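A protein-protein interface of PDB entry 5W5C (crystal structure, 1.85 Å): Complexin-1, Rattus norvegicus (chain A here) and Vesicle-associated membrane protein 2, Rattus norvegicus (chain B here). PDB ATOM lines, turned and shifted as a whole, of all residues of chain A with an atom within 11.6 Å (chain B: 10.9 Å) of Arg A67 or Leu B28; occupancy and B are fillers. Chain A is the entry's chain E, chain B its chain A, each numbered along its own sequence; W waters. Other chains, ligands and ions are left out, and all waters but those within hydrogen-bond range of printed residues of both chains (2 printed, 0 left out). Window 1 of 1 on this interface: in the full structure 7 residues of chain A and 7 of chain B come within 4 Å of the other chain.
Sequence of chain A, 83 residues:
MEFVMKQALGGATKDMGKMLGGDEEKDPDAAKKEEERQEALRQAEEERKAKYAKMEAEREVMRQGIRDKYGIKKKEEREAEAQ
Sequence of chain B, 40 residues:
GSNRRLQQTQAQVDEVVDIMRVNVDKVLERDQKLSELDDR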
ATOM      1  N   GLU A  56     -14.310 -12.772 -35.550  1.00  0.00           N
ATOM      2  CA  GLU A  56     -14.132 -11.360 -35.227  1.00  0.00           C
ATOM      3  C   GLU A  56     -15.352 -10.803 -34.502  1.00  0.00           C
ATOM      4  O   GLU A  56     -15.218  -9.962 -33.598  1.00  0.00           O
ATOM      5  CB  GLU A  56     -13.844 -10.558 -36.499  1.00  0.00           C
ATOM      6  CG  GLU A  56     -13.563  -9.063 -36.265  1.00  0.00           C
ATOM      7  CD  GLU A  56     -12.625  -8.785 -35.081  1.00  0.00           C
ATOM      8  OE1 GLU A  56     -12.898  -7.851 -34.291  1.00  0.00           O
ATOM      9  OE2 GLU A  56     -11.608  -9.497 -34.946  1.00  0.00           O
ATOM     10  N   GLU A  58     -17.371 -12.847 -32.726  1.00  0.00           N
ATOM     11  CA  GLU A  58     -17.209 -13.519 -31.440  1.00  0.00           C
ATOM     12  C   GLU A  58     -16.218 -12.768 -30.554  1.00  0.00           C
ATOM     13  O   GLU A  58     -16.487 -12.520 -29.369  1.00  0.00           O
ATOM     14  CB  GLU A  58     -16.761 -14.968 -31.655  1.00  0.00           C
ATOM     15  N   ARG A  59     -15.089 -12.355 -31.133  1.00  0.00           N
ATOM     16  CA  ARG A  59     -14.071 -11.631 -30.383  1.00  0.00           C
ATOM     17  C   ARG A  59     -14.605 -10.299 -29.871  1.00  0.00           C
ATOM     18  O   ARG A  59     -14.374  -9.932 -28.712  1.00  0.00           O
ATOM     19  CB  ARG A  59     -12.819 -11.428 -31.254  1.00  0.00           C
ATOM     20  CG  ARG A  59     -11.677 -10.682 -30.553  1.00  0.00           C
ATOM     21  CD  ARG A  59     -10.291 -11.103 -31.055  1.00  0.00           C
ATOM     22  NE  ARG A  59      -9.278 -10.739 -30.076  1.00  0.00           N
ATOM     23  CZ  ARG A  59      -8.729 -11.589 -29.205  1.00  0.00           C
ATOM     24  NH1 ARG A  59      -9.080 -12.862 -29.173  1.00  0.00           N
ATOM     25  NH2 ARG A  59      -7.845 -11.151 -28.338  1.00  0.00           N
ATOM     26  N   GLU A  60     -15.324  -9.556 -30.711  1.00  0.00           N
ATOM     27  CA  GLU A  60     -15.901  -8.309 -30.222  1.00  0.00           C
ATOM     28  C   GLU A  60     -16.891  -8.558 -29.077  1.00  0.00           C
ATOM     29  O   GLU A  60     -17.066  -7.699 -28.201  1.00  0.00           O
ATOM     30  CB  GLU A  60     -16.561  -7.557 -31.373  1.00  0.00           C
ATOM     31  CG  GLU A  60     -17.284  -6.296 -30.948  1.00  0.00           C
ATOM     32  CD  GLU A  60     -16.426  -5.369 -30.116  1.00  0.00           C
ATOM     33  OE1 GLU A  60     -15.206  -5.269 -30.390  1.00  0.00           O
ATOM     34  OE2 GLU A  60     -16.976  -4.727 -29.189  1.00  0.00           O
ATOM     35  N   VAL A  61     -17.501  -9.746 -29.035  1.00  0.00           N
ATOM     36  CA  VAL A  61     -18.341 -10.085 -27.885  1.00  0.00           C
ATOM     37  C   VAL A  61     -17.482 -10.321 -26.641  1.00  0.00           C
ATOM     38  O   VAL A  61     -17.817  -9.844 -25.547  1.00  0.00           O
ATOM     39  CB  VAL A  61     -19.244 -11.293 -28.224  1.00  0.00           C
ATOM     40  CG1 VAL A  61     -19.733 -12.018 -26.974  1.00  0.00           C
ATOM     41  CG2 VAL A  61     -20.424 -10.815 -29.059  1.00  0.00           C
ATOM     42  N   MET A  62     -16.359 -11.047 -26.789  1.00  0.00           N
ATOM     43  CA  MET A  62     -15.368 -11.152 -25.711  1.00  0.00           C
ATOM     44  C   MET A  62     -14.932  -9.777 -25.183  1.00  0.00           C
ATOM     45  O   MET A  62     -14.921  -9.545 -23.958  1.00  0.00           O
ATOM     46  CB  MET A  62     -14.174 -11.980 -26.214  1.00  0.00           C
ATOM     47  CG  MET A  62     -13.160 -12.379 -25.126  1.00  0.00           C
ATOM     48  SD  MET A  62     -11.845 -11.135 -25.149  1.00  0.00           S
ATOM     49  CE  MET A  62     -11.277 -11.292 -26.846  1.00  0.00           C
ATOM     50  N   ARG A  63     -14.693  -8.814 -26.092  1.00  0.00           N
ATOM     51  CA  ARG A  63     -14.254  -7.468 -25.715  1.00  0.00           C
ATOM     52  C   ARG A  63     -15.303  -6.721 -24.912  1.00  0.00           C
ATOM     53  O   ARG A  63     -14.992  -6.027 -23.915  1.00  0.00           O
ATOM     54  CB  ARG A  63     -13.929  -6.643 -26.967  1.00  0.00           C
ATOM     55  CG  ARG A  63     -12.625  -6.989 -27.680  1.00  0.00           C
ATOM     56  CD  ARG A  63     -12.251  -5.940 -28.765  1.00  0.00           C
ATOM     57  NE  ARG A  63     -11.466  -6.646 -29.764  1.00  0.00           N
ATOM     58  CZ  ARG A  63     -11.845  -6.868 -31.016  1.00  0.00           C
ATOM     59  NH1 ARG A  63     -13.002  -6.390 -31.445  1.00  0.00           N
ATOM     60  NH2 ARG A  63     -11.055  -7.571 -31.837  1.00  0.00           N
ATOM     61  N   GLN A  64     -16.538  -6.706 -25.428  1.00  0.00           N
ATOM     62  CA  GLN A  64     -17.599  -6.055 -24.668  1.00  0.00           C
ATOM     63  C   GLN A  64     -17.822  -6.746 -23.337  1.00  0.00           C
ATOM     64  O   GLN A  64     -18.120  -6.081 -22.341  1.00  0.00           O
ATOM     65  CB  GLN A  64     -18.893  -6.011 -25.468  1.00  0.00           C
ATOM     66  CG  GLN A  64     -19.893  -5.061 -24.798  1.00  0.00           C
ATOM     67  CD  GLN A  64     -19.397  -3.652 -24.665  1.00  0.00           C
ATOM     68  OE1 GLN A  64     -18.843  -3.112 -25.602  1.00  0.00           O
ATOM     69  NE2 GLN A  64     -19.669  -3.005 -23.516  1.00  0.00           N
ATOM     70  N   GLY A  65     -17.632  -8.067 -23.300  1.00  0.00           N
ATOM     71  CA  GLY A  65     -17.620  -8.789 -22.040  1.00  0.00           C
ATOM     72  C   GLY A  65     -16.703  -8.153 -21.022  1.00  0.00           C
ATOM     73  O   GLY A  65     -17.126  -7.810 -19.915  1.00  0.00           O
ATOM     74  N   ILE A  66     -15.440  -7.912 -21.408  1.00  0.00           N
ATOM     75  CA  ILE A  66     -14.486  -7.356 -20.443  1.00  0.00           C
ATOM     76  C   ILE A  66     -14.908  -5.992 -19.988  1.00  0.00           C
ATOM     77  O   ILE A  66     -14.885  -5.678 -18.782  1.00  0.00           O
ATOM     78  CB  ILE A  66     -13.070  -7.261 -21.057  1.00  0.00           C
ATOM     79  CG1 ILE A  66     -12.705  -8.534 -21.720  1.00  0.00           C
ATOM     80  CG2 ILE A  66     -12.053  -6.951 -19.989  1.00  0.00           C
ATOM     81  CD1 ILE A  66     -12.527  -9.672 -20.752  1.00  0.00           C
ATOM     82  N   ARG A  67     -15.268  -5.126 -20.956  1.00  0.00           N
ATOM     83  CA  ARG A  67     -15.705  -3.789 -20.602  1.00  0.00           C
ATOM     84  C   ARG A  67     -16.871  -3.822 -19.615  1.00  0.00           C
ATOM     85  O   ARG A  67     -16.911  -3.023 -18.657  1.00  0.00           O
ATOM     86  CB  ARG A  67     -16.093  -3.015 -21.865  1.00  0.00           C
ATOM     87  CG  ARG A  67     -15.023  -3.027 -22.957  1.00  0.00           C
ATOM     88  CD  ARG A  67     -15.138  -1.823 -23.920  1.00  0.00           C
ATOM     89  NE  ARG A  67     -13.843  -1.538 -24.543  1.00  0.00           N
ATOM     90  CZ  ARG A  67     -13.168  -0.397 -24.400  1.00  0.00           C
ATOM     91  NH1 ARG A  67     -13.689   0.598 -23.684  1.00  0.00           N
ATOM     92  NH2 ARG A  67     -11.978  -0.237 -24.991  1.00  0.00           N
ATOM     93  N   ASP A  68     -17.843  -4.716 -19.848  1.00  0.00           N
ATOM     94  CA  ASP A  68     -19.025  -4.822 -18.982  1.00  0.00           C
ATOM     95  C   ASP A  68     -18.609  -5.273 -17.602  1.00  0.00           C
ATOM     96  O   ASP A  68     -19.036  -4.733 -16.574  1.00  0.00           O
ATOM     97  CB  ASP A  68     -20.018  -5.879 -19.517  1.00  0.00           C
ATOM     98  CG  ASP A  68     -20.801  -5.463 -20.760  1.00  0.00           C
ATOM     99  OD1 ASP A  68     -20.971  -4.244 -21.057  1.00  0.00           O
ATOM    100  OD2 ASP A  68     -21.326  -6.420 -21.419  1.00  0.00           O
ATOM    101  N   LYS A  69     -17.773  -6.308 -17.580  1.00  0.00           N
ATOM    102  CA  LYS A  69     -17.353  -6.906 -16.323  1.00  0.00           C
ATOM    103  C   LYS A  69     -16.748  -5.856 -15.396  1.00  0.00           C
ATOM    104  O   LYS A  69     -16.928  -5.936 -14.183  1.00  0.00           O
ATOM    105  CB  LYS A  69     -16.324  -8.023 -16.651  1.00  0.00           C
ATOM    106  CG  LYS A  69     -15.644  -8.594 -15.489  1.00  0.00           C
ATOM    107  CD  LYS A  69     -15.069  -9.997 -15.844  1.00  0.00           C
ATOM    108  CE  LYS A  69     -13.667  -9.939 -16.364  1.00  0.00           C
ATOM    109  NZ  LYS A  69     -13.155 -11.389 -16.346  1.00  0.00           N
ATOM    110  N   TYR A  70     -15.925  -4.931 -15.934  1.00  0.00           N
ATOM    111  CA  TYR A  70     -15.224  -3.965 -15.082  1.00  0.00           C
ATOM    112  C   TYR A  70     -15.896  -2.607 -15.053  1.00  0.00           C
ATOM    113  O   TYR A  70     -15.425  -1.714 -14.336  1.00  0.00           O
ATOM    114  CB  TYR A  70     -13.750  -3.734 -15.518  1.00  0.00           C
ATOM    115  CG  TYR A  70     -12.955  -5.035 -15.429  1.00  0.00           C
ATOM    116  CD1 TYR A  70     -12.855  -5.702 -14.224  1.00  0.00           C
ATOM    117  CD2 TYR A  70     -12.402  -5.650 -16.561  1.00  0.00           C
ATOM    118  CE1 TYR A  70     -12.223  -6.920 -14.115  1.00  0.00           C
ATOM    119  CE2 TYR A  70     -11.738  -6.856 -16.440  1.00  0.00           C
ATOM    120  CZ  TYR A  70     -11.637  -7.479 -15.227  1.00  0.00           C
ATOM    121  OH  TYR A  70     -10.960  -8.706 -15.135  1.00  0.00           O
ATOM    122  N   GLY A  71     -16.969  -2.429 -15.804  1.00  0.00           N
ATOM    123  CA  GLY A  71     -17.674  -1.158 -15.752  1.00  0.00           C
ATOM    124  C   GLY A  71     -16.952  -0.127 -16.576  1.00  0.00           C
ATOM    125  O   GLY A  71     -16.819   1.021 -16.148  1.00  0.00           O
ATOM    126  N   ILE A  72     -16.429  -0.525 -17.732  1.00  0.00           N
ATOM    127  CA  ILE A  72     -15.673   0.387 -18.589  1.00  0.00           C
ATOM    128  C   ILE A  72     -16.627   0.994 -19.606  1.00  0.00           C
ATOM    129  O   ILE A  72     -17.409   0.273 -20.245  1.00  0.00           O
ATOM    130  CB  ILE A  72     -14.538  -0.345 -19.304  1.00  0.00           C
ATOM    131  CG1 ILE A  72     -13.454  -0.738 -18.297  1.00  0.00           C
ATOM    132  CG2 ILE A  72     -14.071   0.480 -20.484  1.00  0.00           C
ATOM    133  CD1 ILE A  72     -12.370  -1.631 -18.899  1.00  0.00           C
ATOM    134  N   LYS A  73     -16.588   2.314 -19.735  1.00  0.00           N
ATOM    135  CA  LYS A  73     -17.373   3.025 -20.732  1.00  0.00           C
ATOM    136  C   LYS A  73     -16.502   3.324 -21.948  1.00  0.00           C
ATOM    137  O   LYS A  73     -15.304   3.613 -21.823  1.00  0.00           O
ATOM    138  CB  LYS A  73     -17.955   4.327 -20.160  1.00  0.00           C
ATOM    139  N   LYS A  74     -17.114   3.241 -23.125  1.00  0.00           N
ATOM    140  CA  LYS A  74     -16.438   3.584 -24.365  1.00  0.00           C
ATOM    141  C   LYS A  74     -16.383   5.105 -24.545  1.00  0.00           C
ATOM    142  O   LYS A  74     -17.046   5.873 -23.838  1.00  0.00           O
ATOM    143  CB  LYS A  74     -17.143   2.912 -25.543  1.00  0.00           C
ATOM    144  CG  LYS A  74     -16.660   1.498 -25.786  1.00  0.00           C
ATOM    145  CD  LYS A  74     -17.804   0.518 -25.928  1.00  0.00           C
ATOM    146  CE  LYS A  74     -18.912   1.054 -26.814  1.00  0.00           C
ATOM    147  NZ  LYS A  74     -19.452  -0.096 -27.618  1.00  0.00           N
ATOM    148  N   LYS A  75     -15.568   5.540 -25.505  1.00  0.00           N
ATOM    149  CA  LYS A  75     -15.461   6.959 -25.828  1.00  0.00           C
ATOM    150  C   LYS A  75     -16.237   7.278 -27.104  1.00  0.00           C
ATOM    151  O   LYS A  75     -17.415   6.927 -27.235  1.00  0.00           O
ATOM    152  CB  LYS A  75     -13.991   7.368 -25.973  1.00  0.00           C
ATOM    153  N   ILE B  19      -6.186   2.536 -12.053  1.00  0.00           N
ATOM    154  CA  ILE B  19      -5.208   2.565 -13.148  1.00  0.00           C
ATOM    155  C   ILE B  19      -5.437   1.407 -14.110  1.00  0.00           C
ATOM    156  O   ILE B  19      -5.362   1.576 -15.347  1.00  0.00           O
ATOM    157  CB  ILE B  19      -3.760   2.535 -12.589  1.00  0.00           C
ATOM    158  CG1 ILE B  19      -3.499   3.761 -11.729  1.00  0.00           C
ATOM    159  CG2 ILE B  19      -2.768   2.526 -13.767  1.00  0.00           C
ATOM    160  CD1 ILE B  19      -2.295   3.571 -10.796  1.00  0.00           C
ATOM    161  N   MET B  20      -5.682   0.186 -13.579  1.00  0.00           N
ATOM    162  CA  MET B  20      -5.760  -0.958 -14.483  1.00  0.00           C
ATOM    163  C   MET B  20      -7.021  -0.892 -15.309  1.00  0.00           C
ATOM    164  O   MET B  20      -7.048  -1.390 -16.439  1.00  0.00           O
ATOM    165  CB  MET B  20      -5.691  -2.322 -13.725  1.00  0.00           C
ATOM    166  CG  MET B  20      -4.295  -2.583 -13.146  1.00  0.00           C
ATOM    167  SD  MET B  20      -3.166  -2.963 -14.539  1.00  0.00           S
ATOM    168  CE  MET B  20      -3.958  -4.507 -15.126  1.00  0.00           C
ATOM    169  N   ARG B  21      -8.088  -0.317 -14.757  1.00  0.00           N
ATOM    170  CA  ARG B  21      -9.288  -0.141 -15.567  1.00  0.00           C
ATOM    171  C   ARG B  21      -8.971   0.695 -16.801  1.00  0.00           C
ATOM    172  O   ARG B  21      -9.317   0.308 -17.929  1.00  0.00           O
ATOM    173  CB  ARG B  21     -10.388   0.520 -14.729  1.00  0.00           C
ATOM    174  CG  ARG B  21     -11.734   0.294 -15.399  1.00  0.00           C
ATOM    175  CD  ARG B  21     -12.825   1.078 -14.630  1.00  0.00           C
ATOM    176  NE  ARG B  21     -13.053   0.497 -13.310  1.00  0.00           N
ATOM    177  CZ  ARG B  21     -12.752   1.110 -12.186  1.00  0.00           C
ATOM    178  NH1 ARG B  21     -12.994   0.487 -11.023  1.00  0.00           N
ATOM    179  NH2 ARG B  21     -12.209   2.333 -12.235  1.00  0.00           N
ATOM    180  N   VAL B  22      -8.245   1.811 -16.601  1.00  0.00           N
ATOM    181  CA  VAL B  22      -7.776   2.595 -17.755  1.00  0.00           C
ATOM    182  C   VAL B  22      -6.905   1.737 -18.687  1.00  0.00           C
ATOM    183  O   VAL B  22      -7.093   1.713 -19.923  1.00  0.00           O
ATOM    184  CB  VAL B  22      -7.064   3.867 -17.260  1.00  0.00           C
ATOM    185  CG1 VAL B  22      -6.227   4.523 -18.375  1.00  0.00           C
ATOM    186  CG2 VAL B  22      -8.101   4.856 -16.712  1.00  0.00           C
ATOM    187  N   ASN B  23      -5.982   0.953 -18.110  1.00  0.00           N
ATOM    188  CA  ASN B  23      -5.139   0.090 -18.947  1.00  0.00           C
ATOM    189  C   ASN B  23      -5.940  -0.915 -19.747  1.00  0.00           C
ATOM    190  O   ASN B  23      -5.597  -1.231 -20.898  1.00  0.00           O
ATOM    191  CB  ASN B  23      -4.113  -0.671 -18.067  1.00  0.00           C
ATOM    192  CG  ASN B  23      -3.019   0.246 -17.551  1.00  0.00           C
ATOM    193  OD1 ASN B  23      -2.916   1.395 -17.985  1.00  0.00           O
ATOM    194  ND2 ASN B  23      -2.258  -0.217 -16.538  1.00  0.00           N
ATOM    195  N   VAL B  24      -6.966  -1.505 -19.136  1.00  0.00           N
ATOM    196  CA  VAL B  24      -7.739  -2.538 -19.835  1.00  0.00           C
ATOM    197  C   VAL B  24      -8.498  -1.920 -21.018  1.00  0.00           C
ATOM    198  O   VAL B  24      -8.543  -2.494 -22.119  1.00  0.00           O
ATOM    199  CB  VAL B  24      -8.686  -3.253 -18.852  1.00  0.00           C
ATOM    200  CG1 VAL B  24      -9.762  -4.116 -19.612  1.00  0.00           C
ATOM    201  CG2 VAL B  24      -7.890  -4.172 -17.904  1.00  0.00           C
ATOM    202  N   ASP B  25      -9.089  -0.748 -20.801  1.00  0.00           N
ATOM    203  CA  ASP B  25      -9.648   0.053 -21.906  1.00  0.00           C
ATOM    204  C   ASP B  25      -8.638   0.244 -23.054  1.00  0.00           C
ATOM    205  O   ASP B  25      -8.934  -0.048 -24.232  1.00  0.00           O
ATOM    206  CB  ASP B  25     -10.070   1.410 -21.345  1.00  0.00           C
ATOM    207  CG  ASP B  25     -11.038   2.188 -22.281  1.00  0.00           C
ATOM    208  OD1 ASP B  25     -11.618   1.605 -23.219  1.00  0.00           O
ATOM    209  OD2 ASP B  25     -11.184   3.379 -22.066  1.00  0.00           O
ATOM    210  N   LYS B  26      -7.432   0.762 -22.718  1.00  0.00           N
ATOM    211  CA  LYS B  26      -6.398   0.988 -23.735  1.00  0.00           C
ATOM    212  C   LYS B  26      -6.018  -0.301 -24.452  1.00  0.00           C
ATOM    213  O   LYS B  26      -5.793  -0.303 -25.672  1.00  0.00           O
ATOM    214  CB  LYS B  26      -5.161   1.613 -23.104  1.00  0.00           C
ATOM    215  CG  LYS B  26      -5.316   3.057 -22.679  1.00  0.00           C
ATOM    216  CD  LYS B  26      -4.089   3.488 -21.768  1.00  0.00           C
ATOM    217  CE  LYS B  26      -4.208   4.990 -21.433  1.00  0.00           C
ATOM    218  NZ  LYS B  26      -3.343   5.497 -20.339  1.00  0.00           N
ATOM    219  N   VAL B  27      -5.948  -1.420 -23.728  1.00  0.00           N
ATOM    220  CA  VAL B  27      -5.511  -2.628 -24.428  1.00  0.00           C
ATOM    221  C   VAL B  27      -6.654  -3.233 -25.238  1.00  0.00           C
ATOM    222  O   VAL B  27      -6.390  -4.021 -26.149  1.00  0.00           O
ATOM    223  CB  VAL B  27      -4.907  -3.666 -23.467  1.00  0.00           C
ATOM    224  CG1 VAL B  27      -5.947  -4.540 -22.803  1.00  0.00           C
ATOM    225  CG2 VAL B  27      -3.828  -4.535 -24.188  1.00  0.00           C
ATOM    226  N   LEU B  28      -7.920  -2.902 -24.924  1.00  0.00           N
ATOM    227  CA  LEU B  28      -9.020  -3.290 -25.812  1.00  0.00           C
ATOM    228  C   LEU B  28      -9.018  -2.468 -27.107  1.00  0.00           C
ATOM    229  O   LEU B  28      -9.270  -3.006 -28.191  1.00  0.00           O
ATOM    230  CB  LEU B  28     -10.368  -3.155 -25.068  1.00  0.00           C
ATOM    231  CG  LEU B  28     -10.534  -4.252 -24.009  1.00  0.00           C
ATOM    232  CD1 LEU B  28     -11.802  -4.001 -23.146  1.00  0.00           C
ATOM    233  CD2 LEU B  28     -10.489  -5.671 -24.559  1.00  0.00           C
ATOM    234  N   GLU B  29      -8.727  -1.179 -27.027  1.00  0.00           N
ATOM    235  CA  GLU B  29      -8.399  -0.436 -28.252  1.00  0.00           C
ATOM    236  C   GLU B  29      -7.281  -1.125 -29.028  1.00  0.00           C
ATOM    237  O   GLU B  29      -7.402  -1.405 -30.233  1.00  0.00           O
ATOM    238  CB  GLU B  29      -7.983   0.981 -27.913  1.00  0.00           C
ATOM    239  CG  GLU B  29      -9.134   1.865 -27.355  1.00  0.00           C
ATOM    240  CD  GLU B  29      -8.690   3.277 -26.985  1.00  0.00           C
ATOM    241  OE1 GLU B  29      -7.480   3.482 -26.736  1.00  0.00           O
ATOM    242  OE2 GLU B  29      -9.546   4.180 -26.895  1.00  0.00           O
ATOM    243  N   ARG B  30      -6.197  -1.457 -28.328  1.00  0.00           N
ATOM    244  CA  ARG B  30      -5.085  -2.136 -28.991  1.00  0.00           C
ATOM    245  C   ARG B  30      -5.562  -3.395 -29.687  1.00  0.00           C
ATOM    246  O   ARG B  30      -5.176  -3.667 -30.833  1.00  0.00           O
ATOM    247  CB  ARG B  30      -4.005  -2.432 -27.954  1.00  0.00           C
ATOM    248  CG  ARG B  30      -2.708  -3.059 -28.536  1.00  0.00           C
ATOM    249  CD  ARG B  30      -1.692  -3.272 -27.376  1.00  0.00           C
ATOM    250  NE  ARG B  30      -0.331  -3.565 -27.870  1.00  0.00           N
ATOM    251  CZ  ARG B  30       0.200  -4.776 -27.973  1.00  0.00           C
ATOM    252  NH1 ARG B  30      -0.451  -5.883 -27.623  1.00  0.00           N
ATOM    253  NH2 ARG B  30       1.456  -4.874 -28.412  1.00  0.00           N
ATOM    254  N   ASP B  31      -6.449  -4.151 -29.025  1.00  0.00           N
ATOM    255  CA  ASP B  31      -6.952  -5.400 -29.589  1.00  0.00           C
ATOM    256  C   ASP B  31      -7.739  -5.138 -30.862  1.00  0.00           C
ATOM    257  O   ASP B  31      -7.614  -5.874 -31.847  1.00  0.00           O
ATOM    258  CB  ASP B  31      -7.834  -6.126 -28.564  1.00  0.00           C
ATOM    259  CG  ASP B  31      -8.010  -7.607 -28.877  1.00  0.00           C
ATOM    260  OD1 ASP B  31      -8.929  -7.939 -29.661  1.00  0.00           O
ATOM    261  OD2 ASP B  31      -7.236  -8.459 -28.350  1.00  0.00           O
ATOM    262  N   GLN B  32      -8.559  -4.091 -30.848  1.00  0.00           N
ATOM    263  CA  GLN B  32      -9.333  -3.728 -32.025  1.00  0.00           C
ATOM    264  C   GLN B  32      -8.416  -3.412 -33.208  1.00  0.00           C
ATOM    265  O   GLN B  32      -8.527  -4.032 -34.275  1.00  0.00           O
ATOM    266  CB  GLN B  32     -10.235  -2.542 -31.676  1.00  0.00           C
ATOM    267  CG  GLN B  32     -11.090  -2.027 -32.804  1.00  0.00           C
ATOM    268  CD  GLN B  32     -10.730  -0.600 -33.178  1.00  0.00           C
ATOM    269  OE1 GLN B  32     -10.288   0.193 -32.331  1.00  0.00           O
ATOM    270  NE2 GLN B  32     -10.899  -0.270 -34.455  1.00  0.00           N
ATOM    271  N   LYS B  33      -7.466  -2.487 -33.016  1.00  0.00           N
ATOM    272  CA  LYS B  33      -6.570  -2.094 -34.106  1.00  0.00           C
ATOM    273  C   LYS B  33      -5.752  -3.272 -34.648  1.00  0.00           C
ATOM    274  O   LYS B  33      -5.619  -3.439 -35.868  1.00  0.00           O
ATOM    275  CB  LYS B  33      -5.662  -0.984 -33.615  1.00  0.00           C
ATOM    276  CG  LYS B  33      -6.433   0.162 -33.001  1.00  0.00           C
ATOM    277  CD  LYS B  33      -5.507   1.307 -32.587  1.00  0.00           C
ATOM    278  CE  LYS B  33      -6.340   2.523 -32.183  1.00  0.00           C
ATOM    279  NZ  LYS B  33      -5.530   3.733 -31.920  1.00  0.00           N
ATOM    280  N   LEU B  34      -5.230  -4.122 -33.764  1.00  0.00           N
ATOM    281  CA  LEU B  34      -4.416  -5.242 -34.214  1.00  0.00           C
ATOM    282  C   LEU B  34      -5.247  -6.309 -34.927  1.00  0.00           C
ATOM    283  O   LEU B  34      -4.799  -6.883 -35.925  1.00  0.00           O
ATOM    284  CB  LEU B  34      -3.692  -5.860 -33.025  1.00  0.00           C
ATOM    285  CG  LEU B  34      -2.579  -5.029 -32.398  1.00  0.00           C
ATOM    286  CD1 LEU B  34      -2.071  -5.867 -31.249  1.00  0.00           C
ATOM    287  CD2 LEU B  34      -1.469  -4.752 -33.437  1.00  0.00           C
ATOM    288  N   SER B  35      -6.427  -6.644 -34.389  1.00  0.00           N
ATOM    289  CA  SER B  35      -7.345  -7.535 -35.098  1.00  0.00           C
ATOM    290  C   SER B  35      -7.641  -7.006 -36.496  1.00  0.00           C
ATOM    291  O   SER B  35      -7.675  -7.771 -37.469  1.00  0.00           O
ATOM    292  CB  SER B  35      -8.654  -7.686 -34.312  1.00  0.00           C
ATOM    293  OG  SER B  35      -8.450  -8.371 -33.089  1.00  0.00           O
ATOM    294  N   GLU B  36      -7.855  -5.693 -36.614  1.00  0.00           N
ATOM    295  CA  GLU B  36      -7.993  -5.081 -37.928  1.00  0.00           C
ATOM    296  C   GLU B  36      -6.773  -5.384 -38.804  1.00  0.00           C
ATOM    297  O   GLU B  36      -6.898  -5.968 -39.888  1.00  0.00           O
ATOM    298  CB  GLU B  36      -8.203  -3.582 -37.769  1.00  0.00           C
ATOM    299  CG  GLU B  36      -8.539  -2.862 -39.045  1.00  0.00           C
ATOM    300  CD  GLU B  36      -9.124  -1.488 -38.790  1.00  0.00           C
ATOM    301  OE1 GLU B  36      -9.763  -1.303 -37.726  1.00  0.00           O
ATOM    302  OE2 GLU B  36      -8.935  -0.597 -39.651  1.00  0.00           O
HETATM  303  O   HOH W   1     -16.376   0.359 -12.665  1.00  0.00           O
HETATM  304  O   HOH W   2     -13.898  -1.815 -11.742  1.00  0.00           O
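O of Tyr A70 sits at hydrogen-bond distance from NE of Arg B21, 3.4 Å away.
OD2 of Asp B31 is in salt-bridge range of NH2 of Arg A59 (2.8 Å).
The side-chain hydroxyl (OG) of Ser B35 lies within hydrogen-bond range of the guanidinium group (NH2) of Arg A63 (3.0 Å).
NE of Arg A63 is in salt-bridge range of OD1 of Asp B31, 2.8 Å away.
The side-chain carboxylate of Asp B25 lies within salt-bridge range of the guanidinium group of Arg A67.
The side-chain hydroxyl (OG) of Ser B35 lies within hydrogen-bond range of the backbone carbonyl oxygen (O) of Asp B31.
The side-chain carboxylate of Glu A56 lies within salt-bridge range of the guanidinium group of Arg A63 (3.1 Å).
O of Arg A67 lies within hydrogen-bond range of N of Ile A72.
OE1 of Glu A60 lies within salt-bridge range of NH1 of Arg A63 (2.7 Å).
CB of Ser B35 touches OE2 of Glu A56, at 3.5 Å.
Arg A59 touches Ser B35 (CD to OG, 3.9 Å).
CD1 of Leu B28 touches O of Arg A63, 3.9 Å away.
Ile A66 touches Val B24 (CG2 to CG1, 3.7 Å).
Arg A67 touches Leu B28 (NH2 to CB, 3.3 Å).
NH2 of Arg A67 touches N of Glu B29 (3.9 Å).
CG of Arg B21 touches CG1 of Ile A72, at 3.5 Å.
Ile A72 touches Val B24 (CD1 to CG1, 3.7 Å).
Asp B25 touches Ile A72 (OD1 to CG2, 3.8 Å).
Of the printed residues of chain B, Glu A56 touches Ser B35.
Printed residues of chain B within 4 Å of Arg A59: Asp B31 and Ser B35.
Gln A64 touches none of the printed residues of chain B.
No residue of chain B comes within 4 Å of Gly A65.
Of chain B, only Val B24 (3.7 Å) comes within 4 Å of Ile A66.
Of the printed residues of chain B, Arg A67 touches Asp B25, Leu B28 and Glu B29.
No residue of chain B comes within 4 Å of Asp A68.
Ile A72 touches three residues of chain B.
Lys A73 touches none of the printed residues of chain B.
Lys A74 touches none of the printed residues of chain B.
Of the printed residues of chain A, Arg B21 touches Tyr A70 and Ile A72.
Val B24 touches just these residues of chain A: Ile A66 (3.7 Å) and Ile A72 (3.7 Å).
No residue of chain A comes within 4 Å of Val B27.
Of the printed residues of chain A, Leu B28 touches Arg A63 (3.9 Å) and Arg A67 (3.3 Å).
Of the printed residues of chain A, Ser B35 touches Glu A56, Arg A59 and Arg A63.
The nearest printed residue of chain B that does not touch Arg A67 is Val B24 (5.0 Å).
The nearest printed residue of chain A that does not touch Leu B28 is Ile A66 (4.1 Å).
The nearest printed residue of chain A that does not touch Arg B21 is Gly A71 (4.3 Å).
Hydrophobic or aromatic side chains of chain A within 4 Å of the printed part of chain B: Ile A66 and Ile A72.
Printed residues of chain B that touch a printed residue of chain A: Arg B21, Val B24, Asp B25, Leu B28, Glu B29, Asp B31 and Ser B35.
Hydrophobic or aromatic side chains of chain B that line the printed part of chain A: Val B24 and Leu B28.
Water W2 lies within hydrogen-bond range of NH1 of Arg B21 (2.6 Å) and O of Tyr A70 (3.0 Å).
Water W1 lies within hydrogen-bond range of the backbone carbonyl oxygen (O) of Tyr A70 and the guanidinium group (NE) of Arg B21.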
